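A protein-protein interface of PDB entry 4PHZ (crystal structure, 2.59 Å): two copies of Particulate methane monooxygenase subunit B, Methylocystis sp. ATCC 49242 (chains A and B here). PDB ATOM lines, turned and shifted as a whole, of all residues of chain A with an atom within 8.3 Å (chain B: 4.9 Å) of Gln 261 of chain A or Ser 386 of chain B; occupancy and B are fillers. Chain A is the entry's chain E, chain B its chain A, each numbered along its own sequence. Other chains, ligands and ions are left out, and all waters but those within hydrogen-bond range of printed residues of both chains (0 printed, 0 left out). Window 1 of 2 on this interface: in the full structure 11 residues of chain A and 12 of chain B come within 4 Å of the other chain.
Pro 412 of chain B touches Leu 169 of chain A (O to CD1, 3.3 Å).
Asp 383 of chain B touches Pro 259 of chain A (O to CG, 3.2 Å).
O of Asp 383 of chain B touches NE2 of Gln 261 of chain A, 3.5 Å away.
OE1 of Gln 261 of chain A touches CA of Asp 385 of chain B, at 3.3 Å.
No position is printed for both chains.
Printed residues of chain A that touch a printed residue of chain B: Arg 108, Leu 169, Pro 259, Leu 260, Gln 261 and Ala 262.
Hydrophobic or aromatic side chains of chain A within 4 Å of the printed part of chain B: Leu 169 and Pro 259.
Of the printed residues of chain B, Pro 259 of chain A touches Asp 383 (3.2 Å).
Of the printed residues of chain B, Ala 262 of chain A touches Thr 384.
Gly 263 of chain A touches none of the printed residues of chain B.
Of the printed residues of chain A, Asp 385 of chain B touches Arg 108 and Gln 261.
Gly 408 of chain B touches none of the printed residues of chain A.
Of the printed residues of chain A, Pro 412 of chain B touches Leu 169 (3.3 Å).
The nearest printed residue of chain B that does not touch Gln 261 of chain A is Gln 387 of chain B (6.2 Å).
OG of Ser 386 of chain B sits at hydrogen-bond distance from OH of Tyr 293 of chain B (2.9 Å).
The side-chain carboxylate of Asp 385 of chain B lies close to the side-chain amide oxygen of Gln 387 of chain B (2.8 Å).
N of Val 410 of chain B is in hydrogen-bond range of O of Ser 386 of chain B (3.2 Å).
The guanidinium group (NE) of Arg 108 of chain A sits at hydrogen-bond distance from the backbone carbonyl oxygen (O) of Gly 263 of chain A (2.9 Å).
The side-chain amide nitrogen of Gln 261 of chain A sits at hydrogen-bond distance from the backbone carbonyl oxygen of Pro 259 of chain A, at 2.9 Å.
The side-chain hydroxyl of Thr 384 of chain B lies within hydrogen-bond range of the backbone carbonyl oxygen of Leu 260 of chain A, at 3.2 Å.
The backbone carbonyl oxygen (O) of Thr 384 of chain B sits close to the side-chain amide oxygen (OE1) of Gln 261 of chain A.
The backbone carbonyl oxygen (O) of Thr 384 of chain B is in hydrogen-bond range of the backbone NH (N) of Ala 262 of chain A (3.1 Å).
The side-chain carboxylate (OD2) of Asp 385 of chain B is in salt-bridge range of the guanidinium group (NH2) of Arg 108 of chain A, at 3.1 Å.
The backbone NH (N) of Ser 386 of chain B sits at hydrogen-bond distance from the side-chain amide oxygen (OE1) of Gln 261 of chain A (3.1 Å).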
ATOM      1  N   PRO A 107       3.712 -27.794 -37.077  1.00  0.00           N
ATOM      2  CA  PRO A 107       4.101 -29.125 -36.557  1.00  0.00           C
ATOM      3  C   PRO A 107       2.952 -29.909 -35.882  1.00  0.00           C
ATOM      4  O   PRO A 107       3.074 -31.107 -35.644  1.00  0.00           O
ATOM      5  CB  PRO A 107       5.179 -28.791 -35.514  1.00  0.00           C
ATOM      6  CG  PRO A 107       4.838 -27.398 -35.050  1.00  0.00           C
ATOM      7  CD  PRO A 107       4.148 -26.694 -36.200  1.00  0.00           C
ATOM      8  N   ARG A 108       1.863 -29.229 -35.544  1.00  0.00           N
ATOM      9  CA  ARG A 108       0.748 -29.860 -34.850  1.00  0.00           C
ATOM     10  C   ARG A 108      -0.522 -29.787 -35.674  1.00  0.00           C
ATOM     11  O   ARG A 108      -0.504 -29.323 -36.798  1.00  0.00           O
ATOM     12  CB  ARG A 108       0.578 -29.259 -33.444  1.00  0.00           C
ATOM     13  CG  ARG A 108       1.929 -29.090 -32.775  1.00  0.00           C
ATOM     14  CD  ARG A 108       1.892 -28.948 -31.285  1.00  0.00           C
ATOM     15  NE  ARG A 108       0.908 -27.973 -30.836  1.00  0.00           N
ATOM     16  CZ  ARG A 108       1.177 -26.927 -30.055  1.00  0.00           C
ATOM     17  NH1 ARG A 108       2.420 -26.698 -29.644  1.00  0.00           N
ATOM     18  NH2 ARG A 108       0.189 -26.113 -29.682  1.00  0.00           N
ATOM     19  N   SER A 109      -1.624 -30.259 -35.132  1.00  0.00           N
ATOM     20  CA  SER A 109      -2.832 -30.318 -35.921  1.00  0.00           C
ATOM     21  C   SER A 109      -3.442 -28.911 -36.141  1.00  0.00           C
ATOM     22  O   SER A 109      -3.204 -27.998 -35.342  1.00  0.00           O
ATOM     23  CB  SER A 109      -3.826 -31.287 -35.282  1.00  0.00           C
ATOM     24  OG  SER A 109      -4.063 -30.870 -33.966  1.00  0.00           O
ATOM     25  N   LEU A 169      17.823 -24.479 -26.721  1.00  0.00           N
ATOM     26  CA  LEU A 169      17.572 -23.155 -26.165  1.00  0.00           C
ATOM     27  C   LEU A 169      18.793 -22.584 -25.465  1.00  0.00           C
ATOM     28  O   LEU A 169      19.013 -21.368 -25.469  1.00  0.00           O
ATOM     29  CB  LEU A 169      16.453 -23.195 -25.159  1.00  0.00           C
ATOM     30  CG  LEU A 169      15.004 -22.908 -25.535  1.00  0.00           C
ATOM     31  CD1 LEU A 169      14.294 -22.391 -24.289  1.00  0.00           C
ATOM     32  CD2 LEU A 169      14.794 -21.912 -26.662  1.00  0.00           C
ATOM     33  N   THR A 257      13.910 -29.160 -18.369  1.00  0.00           N
ATOM     34  CA  THR A 257      13.197 -29.906 -19.396  1.00  0.00           C
ATOM     35  C   THR A 257      11.730 -29.464 -19.441  1.00  0.00           C
ATOM     36  O   THR A 257      11.182 -28.912 -18.470  1.00  0.00           O
ATOM     37  CB  THR A 257      13.291 -31.455 -19.212  1.00  0.00           C
ATOM     38  OG1 THR A 257      13.107 -31.830 -17.842  1.00  0.00           O
ATOM     39  CG2 THR A 257      14.632 -32.003 -19.674  1.00  0.00           C
ATOM     40  N   ILE A 258      11.093 -29.704 -20.576  1.00  0.00           N
ATOM     41  CA  ILE A 258       9.714 -29.287 -20.771  1.00  0.00           C
ATOM     42  C   ILE A 258       8.876 -30.525 -21.136  1.00  0.00           C
ATOM     43  O   ILE A 258       9.443 -31.536 -21.628  1.00  0.00           O
ATOM     44  CB  ILE A 258       9.611 -28.184 -21.863  1.00  0.00           C
ATOM     45  CG1 ILE A 258      10.538 -28.488 -23.058  1.00  0.00           C
ATOM     46  CG2 ILE A 258       9.954 -26.827 -21.276  1.00  0.00           C
ATOM     47  CD1 ILE A 258      10.079 -27.883 -24.370  1.00  0.00           C
ATOM     48  N   PRO A 259       7.542 -30.471 -20.880  1.00  0.00           N
ATOM     49  CA  PRO A 259       6.656 -31.545 -21.336  1.00  0.00           C
ATOM     50  C   PRO A 259       6.453 -31.494 -22.854  1.00  0.00           C
ATOM     51  O   PRO A 259       6.536 -30.410 -23.426  1.00  0.00           O
ATOM     52  CB  PRO A 259       5.334 -31.236 -20.616  1.00  0.00           C
ATOM     53  CG  PRO A 259       5.390 -29.782 -20.294  1.00  0.00           C
ATOM     54  CD  PRO A 259       6.826 -29.464 -20.065  1.00  0.00           C
ATOM     55  N   LEU A 260       6.209 -32.634 -23.506  1.00  0.00           N
ATOM     56  CA  LEU A 260       5.805 -32.608 -24.913  1.00  0.00           C
ATOM     57  C   LEU A 260       4.783 -31.482 -25.185  1.00  0.00           C
ATOM     58  O   LEU A 260       3.776 -31.276 -24.448  1.00  0.00           O
ATOM     59  CB  LEU A 260       5.173 -33.929 -25.375  1.00  0.00           C
ATOM     60  CG  LEU A 260       5.870 -35.290 -25.419  1.00  0.00           C
ATOM     61  CD1 LEU A 260       7.152 -35.347 -26.251  1.00  0.00           C
ATOM     62  CD2 LEU A 260       6.168 -35.680 -23.992  1.00  0.00           C
ATOM     63  N   GLN A 261       5.046 -30.771 -26.271  1.00  0.00           N
ATOM     64  CA  GLN A 261       4.181 -29.703 -26.709  1.00  0.00           C
ATOM     65  C   GLN A 261       3.112 -30.277 -27.661  1.00  0.00           C
ATOM     66  O   GLN A 261       3.428 -30.862 -28.692  1.00  0.00           O
ATOM     67  CB  GLN A 261       5.052 -28.602 -27.345  1.00  0.00           C
ATOM     68  CG  GLN A 261       6.077 -28.013 -26.365  1.00  0.00           C
ATOM     69  CD  GLN A 261       5.403 -27.264 -25.216  1.00  0.00           C
ATOM     70  OE1 GLN A 261       4.594 -26.337 -25.428  1.00  0.00           O
ATOM     71  NE2 GLN A 261       5.714 -27.670 -23.995  1.00  0.00           N
ATOM     72  N   ALA A 262       1.845 -30.119 -27.291  1.00  0.00           N
ATOM     73  CA  ALA A 262       0.745 -30.809 -27.972  1.00  0.00           C
ATOM     74  C   ALA A 262      -0.504 -29.945 -27.982  1.00  0.00           C
ATOM     75  O   ALA A 262      -0.739 -29.177 -27.043  1.00  0.00           O
ATOM     76  CB  ALA A 262       0.455 -32.129 -27.281  1.00  0.00           C
ATOM     77  N   GLY A 263      -1.297 -30.070 -29.046  1.00  0.00           N
ATOM     78  CA  GLY A 263      -2.583 -29.380 -29.108  1.00  0.00           C
ATOM     79  C   GLY A 263      -2.855 -28.750 -30.454  1.00  0.00           C
ATOM     80  O   GLY A 263      -1.923 -28.476 -31.243  1.00  0.00           O
ATOM     81  N   LEU A 264      -4.144 -28.502 -30.706  1.00  0.00           N
ATOM     82  CA  LEU A 264      -4.616 -27.918 -31.953  1.00  0.00           C
ATOM     83  C   LEU A 264      -4.113 -26.472 -32.037  1.00  0.00           C
ATOM     84  O   LEU A 264      -4.064 -25.783 -31.014  1.00  0.00           O
ATOM     85  CB  LEU A 264      -6.144 -27.975 -32.014  1.00  0.00           C
ATOM     86  CG  LEU A 264      -6.822 -27.699 -33.352  1.00  0.00           C
ATOM     87  CD1 LEU A 264      -6.538 -28.732 -34.446  1.00  0.00           C
ATOM     88  CD2 LEU A 264      -8.312 -27.536 -33.137  1.00  0.00           C
ATOM     89  N   TYR B 293      10.074 -15.204 -21.517  1.00  0.00           N
ATOM     90  CA  TYR B 293       9.802 -15.157 -20.088  1.00  0.00           C
ATOM     91  C   TYR B 293      10.922 -15.858 -19.341  1.00  0.00           C
ATOM     92  O   TYR B 293      11.538 -16.805 -19.851  1.00  0.00           O
ATOM     93  CB  TYR B 293       8.401 -15.705 -19.727  1.00  0.00           C
ATOM     94  CG  TYR B 293       8.160 -17.188 -19.988  1.00  0.00           C
ATOM     95  CD1 TYR B 293       8.049 -17.689 -21.295  1.00  0.00           C
ATOM     96  CD2 TYR B 293       8.003 -18.092 -18.924  1.00  0.00           C
ATOM     97  CE1 TYR B 293       7.820 -19.046 -21.528  1.00  0.00           C
ATOM     98  CE2 TYR B 293       7.780 -19.451 -19.153  1.00  0.00           C
ATOM     99  CZ  TYR B 293       7.690 -19.920 -20.448  1.00  0.00           C
ATOM    100  OH  TYR B 293       7.472 -21.255 -20.665  1.00  0.00           O
ATOM    101  N   LEU B 380       4.177 -21.528 -16.549  1.00  0.00           N
ATOM    102  CA  LEU B 380       3.873 -21.781 -17.927  1.00  0.00           C
ATOM    103  C   LEU B 380       4.976 -22.694 -18.525  1.00  0.00           C
ATOM    104  O   LEU B 380       4.772 -23.387 -19.548  1.00  0.00           O
ATOM    105  CB  LEU B 380       3.755 -20.430 -18.627  1.00  0.00           C
ATOM    106  CG  LEU B 380       3.807 -20.278 -20.128  1.00  0.00           C
ATOM    107  CD1 LEU B 380       2.707 -21.071 -20.819  1.00  0.00           C
ATOM    108  CD2 LEU B 380       3.632 -18.805 -20.379  1.00  0.00           C
ATOM    109  N   ASP B 383       3.590 -26.082 -18.297  1.00  0.00           N
ATOM    110  CA  ASP B 383       2.508 -26.382 -19.218  1.00  0.00           C
ATOM    111  C   ASP B 383       2.929 -27.018 -20.518  1.00  0.00           C
ATOM    112  O   ASP B 383       4.064 -26.940 -20.977  1.00  0.00           O
ATOM    113  CB  ASP B 383       1.678 -25.149 -19.527  1.00  0.00           C
ATOM    114  CG  ASP B 383       0.901 -24.653 -18.323  1.00  0.00           C
ATOM    115  OD1 ASP B 383       0.912 -25.331 -17.253  1.00  0.00           O
ATOM    116  OD2 ASP B 383       0.295 -23.561 -18.450  1.00  0.00           O
ATOM    117  N   THR B 384       1.932 -27.620 -21.134  1.00  0.00           N
ATOM    118  CA  THR B 384       2.109 -28.504 -22.271  1.00  0.00           C
ATOM    119  C   THR B 384       1.899 -27.746 -23.621  1.00  0.00           C
ATOM    120  O   THR B 384       2.072 -28.311 -24.733  1.00  0.00           O
ATOM    121  CB  THR B 384       1.224 -29.736 -22.084  1.00  0.00           C
ATOM    122  OG1 THR B 384       0.933 -30.242 -23.366  1.00  0.00           O
ATOM    123  CG2 THR B 384      -0.096 -29.388 -21.362  1.00  0.00           C
ATOM    124  N   ASP B 385       1.575 -26.449 -23.476  1.00  0.00           N
ATOM    125  CA  ASP B 385       1.528 -25.462 -24.553  1.00  0.00           C
ATOM    126  C   ASP B 385       2.016 -24.093 -24.058  1.00  0.00           C
ATOM    127  O   ASP B 385       1.268 -23.351 -23.403  1.00  0.00           O
ATOM    128  CB  ASP B 385       0.104 -25.354 -25.080  1.00  0.00           C
ATOM    129  CG  ASP B 385       0.045 -24.812 -26.493  1.00  0.00           C
ATOM    130  OD1 ASP B 385       1.087 -24.324 -26.960  1.00  0.00           O
ATOM    131  OD2 ASP B 385      -1.035 -24.881 -27.144  1.00  0.00           O
ATOM    132  N   SER B 386       3.278 -23.778 -24.354  1.00  0.00           N
ATOM    133  CA  SER B 386       3.943 -22.523 -23.912  1.00  0.00           C
ATOM    134  C   SER B 386       3.518 -21.291 -24.736  1.00  0.00           C
ATOM    135  O   SER B 386       4.075 -20.987 -25.811  1.00  0.00           O
ATOM    136  CB  SER B 386       5.465 -22.689 -23.957  1.00  0.00           C
ATOM    137  OG  SER B 386       6.125 -21.666 -23.241  1.00  0.00           O
ATOM    138  N   GLN B 387       2.533 -20.577 -24.215  1.00  0.00           N
ATOM    139  CA  GLN B 387       1.751 -19.720 -25.045  1.00  0.00           C
ATOM    140  C   GLN B 387       1.002 -18.747 -24.181  1.00  0.00           C
ATOM    141  O   GLN B 387       0.390 -19.128 -23.205  1.00  0.00           O
ATOM    142  CB  GLN B 387       0.776 -20.572 -25.862  1.00  0.00           C
ATOM    143  CG  GLN B 387       0.132 -19.858 -27.038  1.00  0.00           C
ATOM    144  CD  GLN B 387       0.101 -20.727 -28.266  1.00  0.00           C
ATOM    145  OE1 GLN B 387       0.615 -21.846 -28.234  1.00  0.00           O
ATOM    146  NE2 GLN B 387      -0.455 -20.209 -29.375  1.00  0.00           N
ATOM    147  N   ILE B 388       1.044 -17.479 -24.578  1.00  0.00           N
ATOM    148  CA  ILE B 388       0.449 -16.383 -23.816  1.00  0.00           C
ATOM    149  C   ILE B 388      -0.891 -15.981 -24.417  1.00  0.00           C
ATOM    150  O   ILE B 388      -1.150 -16.271 -25.582  1.00  0.00           O
ATOM    151  CB  ILE B 388       1.456 -15.186 -23.754  1.00  0.00           C
ATOM    152  CG1 ILE B 388       1.641 -14.733 -22.317  1.00  0.00           C
ATOM    153  CG2 ILE B 388       1.134 -14.010 -24.707  1.00  0.00           C
ATOM    154  CD1 ILE B 388       2.719 -15.534 -21.629  1.00  0.00           C
ATOM    155  N   GLY B 408      -0.011 -15.841 -28.320  1.00  0.00           N
ATOM    156  CA  GLY B 408       0.851 -16.621 -29.181  1.00  0.00           C
ATOM    157  C   GLY B 408       2.004 -17.217 -28.442  1.00  0.00           C
ATOM    158  O   GLY B 408       2.100 -17.074 -27.215  1.00  0.00           O
ATOM    159  N   PRO B 409       2.871 -17.929 -29.172  1.00  0.00           N
ATOM    160  CA  PRO B 409       3.923 -18.678 -28.494  1.00  0.00           C
ATOM    161  C   PRO B 409       4.877 -17.758 -27.763  1.00  0.00           C
ATOM    162  O   PRO B 409       5.315 -16.749 -28.313  1.00  0.00           O
ATOM    163  CB  PRO B 409       4.658 -19.406 -29.641  1.00  0.00           C
ATOM    164  CG  PRO B 409       4.051 -18.914 -30.920  1.00  0.00           C
ATOM    165  CD  PRO B 409       2.733 -18.289 -30.593  1.00  0.00           C
ATOM    166  N   VAL B 410       5.213 -18.073 -26.524  1.00  0.00           N
ATOM    167  CA  VAL B 410       6.421 -17.455 -25.937  1.00  0.00           C
ATOM    168  C   VAL B 410       7.521 -18.484 -25.617  1.00  0.00           C
ATOM    169  O   VAL B 410       7.253 -19.691 -25.564  1.00  0.00           O
ATOM    170  CB  VAL B 410       6.075 -16.526 -24.765  1.00  0.00           C
ATOM    171  CG1 VAL B 410       5.180 -15.402 -25.262  1.00  0.00           C
ATOM    172  CG2 VAL B 410       5.404 -17.297 -23.645  1.00  0.00           C
ATOM    173  N   PRO B 412      10.778 -19.652 -23.003  1.00  0.00           N
ATOM    174  CA  PRO B 412      11.341 -19.355 -21.699  1.00  0.00           C
ATOM    175  C   PRO B 412      12.870 -19.109 -21.749  1.00  0.00           C
ATOM    176  O   PRO B 412      13.598 -19.678 -22.590  1.00  0.00           O
ATOM    177  CB  PRO B 412      11.018 -20.621 -20.916  1.00  0.00           C
ATOM    178  CG  PRO B 412      11.118 -21.724 -21.946  1.00  0.00           C
ATOM    179  CD  PRO B 412      10.646 -21.111 -23.232  1.00  0.00           C
